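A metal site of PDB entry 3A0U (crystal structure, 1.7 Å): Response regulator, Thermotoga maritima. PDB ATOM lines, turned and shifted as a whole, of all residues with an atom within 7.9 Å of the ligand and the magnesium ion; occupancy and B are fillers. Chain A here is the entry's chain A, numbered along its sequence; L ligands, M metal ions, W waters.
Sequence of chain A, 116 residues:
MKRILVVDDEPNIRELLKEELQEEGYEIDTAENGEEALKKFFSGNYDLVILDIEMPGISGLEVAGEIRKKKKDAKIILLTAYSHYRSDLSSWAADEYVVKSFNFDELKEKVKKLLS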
ATOM      1  N   VAL A   7      26.431  30.922  27.763  1.00  0.00           N
ATOM      2  CA  VAL A   7      26.107  30.781  26.341  1.00  0.00           C
ATOM      3  C   VAL A   7      24.617  30.997  26.117  1.00  0.00           C
ATOM      4  O   VAL A   7      23.806  30.260  26.659  1.00  0.00           O
ATOM      5  CB  VAL A   7      26.463  29.374  25.852  1.00  0.00           C
ATOM      6  CG1 VAL A   7      26.241  29.258  24.339  1.00  0.00           C
ATOM      7  CG2 VAL A   7      27.916  29.008  26.277  1.00  0.00           C
ATOM      8  N   ASP A   8      24.266  32.044  25.384  1.00  0.00           N
ATOM      9  CA  ASP A   8      22.865  32.300  25.105  1.00  0.00           C
ATOM     10  C   ASP A   8      22.811  33.149  23.832  1.00  0.00           C
ATOM     11  O   ASP A   8      23.617  34.066  23.648  1.00  0.00           O
ATOM     12  CB  ASP A   8      22.186  33.007  26.285  1.00  0.00           C
ATOM     13  CG  ASP A   8      20.681  32.963  26.194  1.00  0.00           C
ATOM     14  OD1 ASP A   8      20.125  33.566  25.242  1.00  0.00           O
ATOM     15  OD2 ASP A   8      20.023  32.338  27.071  1.00  0.00           O
ATOM     16  N   ASP A   9      21.840  32.869  22.969  1.00  0.00           N
ATOM     17  CA  ASP A   9      21.748  33.623  21.696  1.00  0.00           C
ATOM     18  C   ASP A   9      21.161  35.026  21.839  1.00  0.00           C
ATOM     19  O   ASP A   9      21.298  35.874  20.937  1.00  0.00           O
ATOM     20  CB  ASP A   9      20.979  32.830  20.617  1.00  0.00           C
ATOM     21  CG  ASP A   9      19.562  32.518  21.009  1.00  0.00           C
ATOM     22  OD1 ASP A   9      19.322  32.116  22.183  1.00  0.00           O
ATOM     23  OD2 ASP A   9      18.653  32.616  20.133  1.00  0.00           O
ATOM     24  N   GLU A  10      20.524  35.296  22.978  1.00  0.00           N
ATOM     25  CA  GLU A  10      19.836  36.568  23.131  1.00  0.00           C
ATOM     26  C   GLU A  10      20.740  37.553  23.890  1.00  0.00           C
ATOM     27  O   GLU A  10      21.048  37.336  25.064  1.00  0.00           O
ATOM     28  CB  GLU A  10      18.493  36.311  23.836  1.00  0.00           C
ATOM     29  CG  GLU A  10      17.580  35.449  22.955  1.00  0.00           C
ATOM     30  CD  GLU A  10      16.189  35.258  23.522  1.00  0.00           C
ATOM     31  OE1 GLU A  10      15.980  34.361  24.347  1.00  0.00           O
ATOM     32  OE2 GLU A  10      15.271  36.002  23.107  1.00  0.00           O
ATOM     33  N   ILE A  13      19.831  38.836  27.319  1.00  0.00           N
ATOM     34  CA  ILE A  13      19.818  37.774  28.333  1.00  0.00           C
ATOM     35  C   ILE A  13      21.245  37.455  28.751  1.00  0.00           C
ATOM     36  O   ILE A  13      21.514  37.269  29.964  1.00  0.00           O
ATOM     37  CB  ILE A  13      19.054  36.510  27.822  1.00  0.00           C
ATOM     38  CG1 ILE A  13      17.591  36.843  27.470  1.00  0.00           C
ATOM     39  CG2 ILE A  13      19.202  35.356  28.847  1.00  0.00           C
ATOM     40  CD1 ILE A  13      16.802  37.653  28.521  1.00  0.00           C
ATOM     41  N   GLU A  32      27.689  33.608  21.882  1.00  0.00           N
ATOM     42  CA  GLU A  32      26.392  33.938  21.304  1.00  0.00           C
ATOM     43  C   GLU A  32      25.720  32.763  20.583  1.00  0.00           C
ATOM     44  O   GLU A  32      24.563  32.846  20.175  1.00  0.00           O
ATOM     45  CB  GLU A  32      26.534  35.124  20.325  1.00  0.00           C
ATOM     46  CG  GLU A  32      27.266  34.795  19.062  1.00  0.00           C
ATOM     47  CD  GLU A  32      27.331  35.972  18.094  1.00  0.00           C
ATOM     48  OE1 GLU A  32      26.929  37.099  18.477  1.00  0.00           O
ATOM     49  OE2 GLU A  32      27.780  35.759  16.944  1.00  0.00           O
ATOM     50  N   LEU A  51      24.465  26.833  29.621  1.00  0.00           N
ATOM     51  CA  LEU A  51      24.120  26.638  28.190  1.00  0.00           C
ATOM     52  C   LEU A  51      22.619  26.820  27.985  1.00  0.00           C
ATOM     53  O   LEU A  51      21.796  26.034  28.491  1.00  0.00           O
ATOM     54  CB  LEU A  51      24.476  25.223  27.706  1.00  0.00           C
ATOM     55  CG  LEU A  51      25.920  24.799  27.543  1.00  0.00           C
ATOM     56  CD1 LEU A  51      25.894  23.344  27.217  1.00  0.00           C
ATOM     57  CD2 LEU A  51      26.643  25.594  26.464  1.00  0.00           C
ATOM     58  N   ASP A  52      22.264  27.850  27.210  1.00  0.00           N
ATOM     59  CA  ASP A  52      20.963  27.931  26.575  1.00  0.00           C
ATOM     60  C   ASP A  52      20.741  26.753  25.642  1.00  0.00           C
ATOM     61  O   ASP A  52      21.680  26.191  25.117  1.00  0.00           O
ATOM     62  CB  ASP A  52      20.936  29.227  25.782  1.00  0.00           C
ATOM     63  CG  ASP A  52      19.573  29.584  25.286  1.00  0.00           C
ATOM     64  OD1 ASP A  52      18.542  29.246  25.932  1.00  0.00           O
ATOM     65  OD2 ASP A  52      19.531  30.226  24.226  1.00  0.00           O
ATOM     66  N   ILE A  53      19.482  26.390  25.425  1.00  0.00           N
ATOM     67  CA  ILE A  53      19.200  25.323  24.488  1.00  0.00           C
ATOM     68  C   ILE A  53      18.858  25.864  23.109  1.00  0.00           C
ATOM     69  O   ILE A  53      19.482  25.462  22.129  1.00  0.00           O
ATOM     70  CB  ILE A  53      18.073  24.392  25.012  1.00  0.00           C
ATOM     71  CG1 ILE A  53      18.561  23.609  26.240  1.00  0.00           C
ATOM     72  CG2 ILE A  53      17.623  23.452  23.886  1.00  0.00           C
ATOM     73  CD1 ILE A  53      17.508  22.719  26.901  1.00  0.00           C
ATOM     74  N   GLU A  54      17.867  26.756  23.016  1.00  0.00           N
ATOM     75  CA  GLU A  54      17.435  27.233  21.709  1.00  0.00           C
ATOM     76  C   GLU A  54      18.323  28.357  21.168  1.00  0.00           C
ATOM     77  O   GLU A  54      18.298  29.513  21.655  1.00  0.00           O
ATOM     78  CB  GLU A  54      15.960  27.675  21.737  1.00  0.00           C
ATOM     79  CG  GLU A  54      15.051  26.521  22.076  1.00  0.00           C
ATOM     80  CD  GLU A  54      13.582  26.860  21.890  1.00  0.00           C
ATOM     81  OE1 GLU A  54      13.269  28.048  21.657  1.00  0.00           O
ATOM     82  OE2 GLU A  54      12.766  25.945  22.041  1.00  0.00           O
ATOM     83  N   MET A  55      19.081  28.014  20.115  1.00  0.00           N
ATOM     84  CA  MET A  55      19.995  28.974  19.483  1.00  0.00           C
ATOM     85  C   MET A  55      20.034  28.728  17.991  1.00  0.00           C
ATOM     86  O   MET A  55      19.771  27.629  17.566  1.00  0.00           O
ATOM     87  CB  MET A  55      21.424  28.786  20.018  1.00  0.00           C
ATOM     88  CG  MET A  55      21.543  29.100  21.520  1.00  0.00           C
ATOM     89  SD  MET A  55      23.211  29.014  22.212  1.00  0.00           S
ATOM     90  CE  MET A  55      23.530  27.270  22.196  1.00  0.00           C
ATOM     91  N   PRO A  56      20.347  29.765  17.204  1.00  0.00           N
ATOM     92  CA  PRO A  56      20.502  29.527  15.773  1.00  0.00           C
ATOM     93  C   PRO A  56      21.737  28.633  15.597  1.00  0.00           C
ATOM     94  O   PRO A  56      22.743  28.811  16.285  1.00  0.00           O
ATOM     95  CB  PRO A  56      20.740  30.928  15.214  1.00  0.00           C
ATOM     96  CG  PRO A  56      20.255  31.897  16.302  1.00  0.00           C
ATOM     97  CD  PRO A  56      20.612  31.169  17.575  1.00  0.00           C
ATOM     98  N   GLY A  60      21.865  23.911  22.344  1.00  0.00           N
ATOM     99  CA  GLY A  60      22.647  23.721  23.562  1.00  0.00           C
ATOM    100  C   GLY A  60      22.677  22.256  24.028  1.00  0.00           C
ATOM    101  O   GLY A  60      23.605  21.851  24.716  1.00  0.00           O
ATOM    102  N   LEU A  78      22.227  23.360  31.971  1.00  0.00           N
ATOM    103  CA  LEU A  78      21.305  23.799  30.915  1.00  0.00           C
ATOM    104  C   LEU A  78      20.415  24.866  31.553  1.00  0.00           C
ATOM    105  O   LEU A  78      19.778  24.590  32.579  1.00  0.00           O
ATOM    106  CB  LEU A  78      20.457  22.629  30.387  1.00  0.00           C
ATOM    107  CG  LEU A  78      21.271  21.655  29.524  1.00  0.00           C
ATOM    108  CD1 LEU A  78      20.516  20.332  29.382  1.00  0.00           C
ATOM    109  CD2 LEU A  78      21.653  22.221  28.148  1.00  0.00           C
ATOM    110  N   LEU A  79      20.404  26.065  30.973  1.00  0.00           N
ATOM    111  CA  LEU A  79      19.563  27.177  31.454  1.00  0.00           C
ATOM    112  C   LEU A  79      18.738  27.654  30.255  1.00  0.00           C
ATOM    113  O   LEU A  79      19.275  28.267  29.330  1.00  0.00           O
ATOM    114  CB  LEU A  79      20.426  28.309  32.017  1.00  0.00           C
ATOM    115  CG  LEU A  79      19.645  29.571  32.440  1.00  0.00           C
ATOM    116  CD1 LEU A  79      18.712  29.258  33.621  1.00  0.00           C
ATOM    117  CD2 LEU A  79      20.622  30.729  32.757  1.00  0.00           C
ATOM    118  N   THR A  80      17.450  27.333  30.286  1.00  0.00           N
ATOM    119  CA  THR A  80      16.567  27.522  29.142  1.00  0.00           C
ATOM    120  C   THR A  80      15.255  28.124  29.608  1.00  0.00           C
ATOM    121  O   THR A  80      14.846  27.910  30.749  1.00  0.00           O
ATOM    122  CB  THR A  80      16.301  26.163  28.417  1.00  0.00           C
ATOM    123  OG1 THR A  80      15.357  26.373  27.347  1.00  0.00           O
ATOM    124  CG2 THR A  80      15.832  25.068  29.399  1.00  0.00           C
ATOM    125  N   ALA A  81      14.608  28.881  28.723  1.00  0.00           N
ATOM    126  CA  ALA A  81      13.301  29.422  29.051  1.00  0.00           C
ATOM    127  C   ALA A  81      12.276  28.302  29.216  1.00  0.00           C
ATOM    128  O   ALA A  81      11.267  28.527  29.880  1.00  0.00           O
ATOM    129  CB  ALA A  81      12.839  30.407  27.991  1.00  0.00           C
ATOM    130  N   TYR A  82      12.523  27.118  28.629  1.00  0.00           N
ATOM    131  CA  TYR A  82      11.474  26.114  28.416  1.00  0.00           C
ATOM    132  C   TYR A  82      11.679  24.841  29.210  1.00  0.00           C
ATOM    133  O   TYR A  82      12.748  24.276  29.202  1.00  0.00           O
ATOM    134  CB  TYR A  82      11.375  25.812  26.915  1.00  0.00           C
ATOM    135  CG  TYR A  82      11.125  27.090  26.122  1.00  0.00           C
ATOM    136  CD1 TYR A  82       9.863  27.724  26.188  1.00  0.00           C
ATOM    137  CD2 TYR A  82      12.151  27.718  25.417  1.00  0.00           C
ATOM    138  CE1 TYR A  82       9.614  28.913  25.529  1.00  0.00           C
ATOM    139  CE2 TYR A  82      11.929  28.923  24.733  1.00  0.00           C
ATOM    140  CZ  TYR A  82      10.641  29.523  24.798  1.00  0.00           C
ATOM    141  OH  TYR A  82      10.371  30.692  24.145  1.00  0.00           O
ATOM    142  N   TYR A  85      12.435  20.473  27.478  1.00  0.00           N
ATOM    143  CA  TYR A  85      13.595  19.609  27.229  1.00  0.00           C
ATOM    144  C   TYR A  85      14.061  18.836  28.453  1.00  0.00           C
ATOM    145  O   TYR A  85      15.008  18.060  28.372  1.00  0.00           O
ATOM    146  CB  TYR A  85      14.755  20.440  26.689  1.00  0.00           C
ATOM    147  CG  TYR A  85      14.403  21.202  25.448  1.00  0.00           C
ATOM    148  CD1 TYR A  85      14.377  20.573  24.224  1.00  0.00           C
ATOM    149  CD2 TYR A  85      14.077  22.552  25.513  1.00  0.00           C
ATOM    150  CE1 TYR A  85      14.023  21.291  23.041  1.00  0.00           C
ATOM    151  CE2 TYR A  85      13.736  23.288  24.376  1.00  0.00           C
ATOM    152  CZ  TYR A  85      13.701  22.632  23.128  1.00  0.00           C
ATOM    153  OH  TYR A  85      13.391  23.332  21.979  1.00  0.00           O
ATOM    154  N   TYR A  97      19.603  21.116  35.250  1.00  0.00           N
ATOM    155  CA  TYR A  97      18.700  21.757  34.292  1.00  0.00           C
ATOM    156  C   TYR A  97      17.890  22.804  35.049  1.00  0.00           C
ATOM    157  O   TYR A  97      17.176  22.476  36.011  1.00  0.00           O
ATOM    158  CB  TYR A  97      17.799  20.712  33.673  1.00  0.00           C
ATOM    159  CG  TYR A  97      16.859  21.125  32.561  1.00  0.00           C
ATOM    160  CD1 TYR A  97      15.730  21.934  32.838  1.00  0.00           C
ATOM    161  CD2 TYR A  97      17.060  20.697  31.267  1.00  0.00           C
ATOM    162  CE1 TYR A  97      14.844  22.301  31.773  1.00  0.00           C
ATOM    163  CE2 TYR A  97      16.198  21.024  30.216  1.00  0.00           C
ATOM    164  CZ  TYR A  97      15.097  21.850  30.468  1.00  0.00           C
ATOM    165  OH  TYR A  97      14.306  22.145  29.381  1.00  0.00           O
ATOM    166  N   VAL A  98      17.979  24.044  34.592  1.00  0.00           N
ATOM    167  CA  VAL A  98      17.289  25.157  35.250  1.00  0.00           C
ATOM    168  C   VAL A  98      16.417  25.890  34.252  1.00  0.00           C
ATOM    169  O   VAL A  98      16.888  26.263  33.169  1.00  0.00           O
ATOM    170  CB  VAL A  98      18.293  26.158  35.871  1.00  0.00           C
ATOM    171  CG1 VAL A  98      17.559  27.357  36.524  1.00  0.00           C
ATOM    172  CG2 VAL A  98      19.149  25.397  36.896  1.00  0.00           C
ATOM    173  N   VAL A  99      15.144  26.084  34.614  1.00  0.00           N
ATOM    174  CA  VAL A  99      14.257  26.915  33.735  1.00  0.00           C
ATOM    175  C   VAL A  99      14.427  28.383  34.133  1.00  0.00           C
ATOM    176  O   VAL A  99      14.291  28.711  35.346  1.00  0.00           O
ATOM    177  CB  VAL A  99      12.762  26.463  33.834  1.00  0.00           C
ATOM    178  CG1 VAL A  99      11.826  27.445  33.179  1.00  0.00           C
ATOM    179  CG2 VAL A  99      12.571  25.050  33.197  1.00  0.00           C
ATOM    180  N   LYS A 100      14.712  29.240  33.174  1.00  0.00           N
ATOM    181  CA  LYS A 100      14.974  30.655  33.456  1.00  0.00           C
ATOM    182  C   LYS A 100      13.842  31.269  34.291  1.00  0.00           C
ATOM    183  O   LYS A 100      12.666  31.121  33.953  1.00  0.00           O
ATOM    184  CB  LYS A 100      15.107  31.458  32.159  1.00  0.00           C
ATOM    185  CG  LYS A 100      16.395  31.200  31.359  1.00  0.00           C
ATOM    186  CD  LYS A 100      16.247  31.757  29.939  1.00  0.00           C
ATOM    187  CE  LYS A 100      17.535  31.587  29.126  1.00  0.00           C
ATOM    188  NZ  LYS A 100      17.398  31.950  27.642  1.00  0.00           N
HETATM  189 BE1  LIG L   1      17.062  29.077  25.493  1.00  0.00          BE
HETATM  190  F1  LIG L   1      16.625  27.448  25.409  1.00  0.00           F
HETATM  191  F2  LIG L   1      16.022  29.787  26.633  1.00  0.00           F
HETATM  192  F3  LIG L   1      16.770  29.886  24.031  1.00  0.00           F
HETATM  193 MG    MG M   1      17.977  30.913  23.113  1.00  0.00          MG
HETATM  194  O   HOH W   1      16.436  31.727  21.939  1.00  0.00           O
HETATM  195  O   HOH W   2      14.437  31.585  24.917  1.00  0.00           O
HETATM  196  O   HOH W   3      17.743  32.459  24.597  1.00  0.00           O
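A beryllium atom (BE1) of the ligand is bound by the side-chain carboxylate (OD1) of Asp 52 (1.6 Å). N of Glu 54 is in hydrogen-bond range of F1 of the ligand (2.8 Å). The side-chain hydroxyl (OG1) of Thr 80 sits at hydrogen-bond distance from a fluorine (F1) of the ligand, 2.6 Å away. The backbone NH (N) of Ala 81 is in hydrogen-bond range of a fluorine (F2) of the ligand, at 2.7 Å. A fluorine (F2) of the ligand sits at hydrogen-bond distance from the side-chain amino group (NZ) of Lys 100 (2.8 Å). A fluorine (F1) of the ligand is in hydrogen-bond range of the backbone NH of Ile 53.
The side-chain carboxylate of Asp 52 sits close to the side-chain amino group of Lys 100, 3.4 Å away. N of Asp 52 is in hydrogen-bond range of O of Val 7, at 2.9 Å. The side-chain carboxylate of Glu 54 sits at hydrogen-bond distance from the side-chain hydroxyl of Tyr 85 (2.7 Å). N of Lys 100 lies within hydrogen-bond range of O of Thr 80 (2.8 Å). The side-chain hydroxyl of Thr 80 lies close to the backbone NH of Tyr 82 (3.2 Å). The backbone NH (N) of Thr 80 lies within hydrogen-bond range of the backbone carbonyl oxygen (O) of Val 98 (3.1 Å). OD2 of Asp 8 lies within salt-bridge range of NZ of Lys 100. The backbone NH (N) of Gly 60 sits at hydrogen-bond distance from the backbone carbonyl oxygen (O) of Ile 53, 2.9 Å away.
Seven residues have an atom within 4 Å of the ligand: Asp 9, Asp 52, Ile 53, Glu 54, Thr 80, Ala 81 and Lys 100.
Along chain A the residues within 4 Å of the magnesium ion span positions 9 to 54.
The magnesium ion is bound by a fluorine (F3) of the ligand, at 1.8 Å. The magnesium ion is bound by OD1 of Asp 9 (2.0 Å). OD2 of Asp 52 is bound to the magnesium ion, 2.0 Å away. O of Glu 54 binds the magnesium ion (2.0 Å). Water W1 binds the magnesium ion. The magnesium ion is bound by water W3 (2.2 Å).
Water W3 lies within hydrogen-bond range of the side-chain carboxylate of Glu 10 (2.6 Å), the side-chain carboxylate of Asp 8 (2.7 Å) and the side-chain amino group of Lys 100 (3.1 Å). Water W2 lies within hydrogen-bond range of F2 of the ligand (2.9 Å) and OE1 of Glu 10 (3.2 Å).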
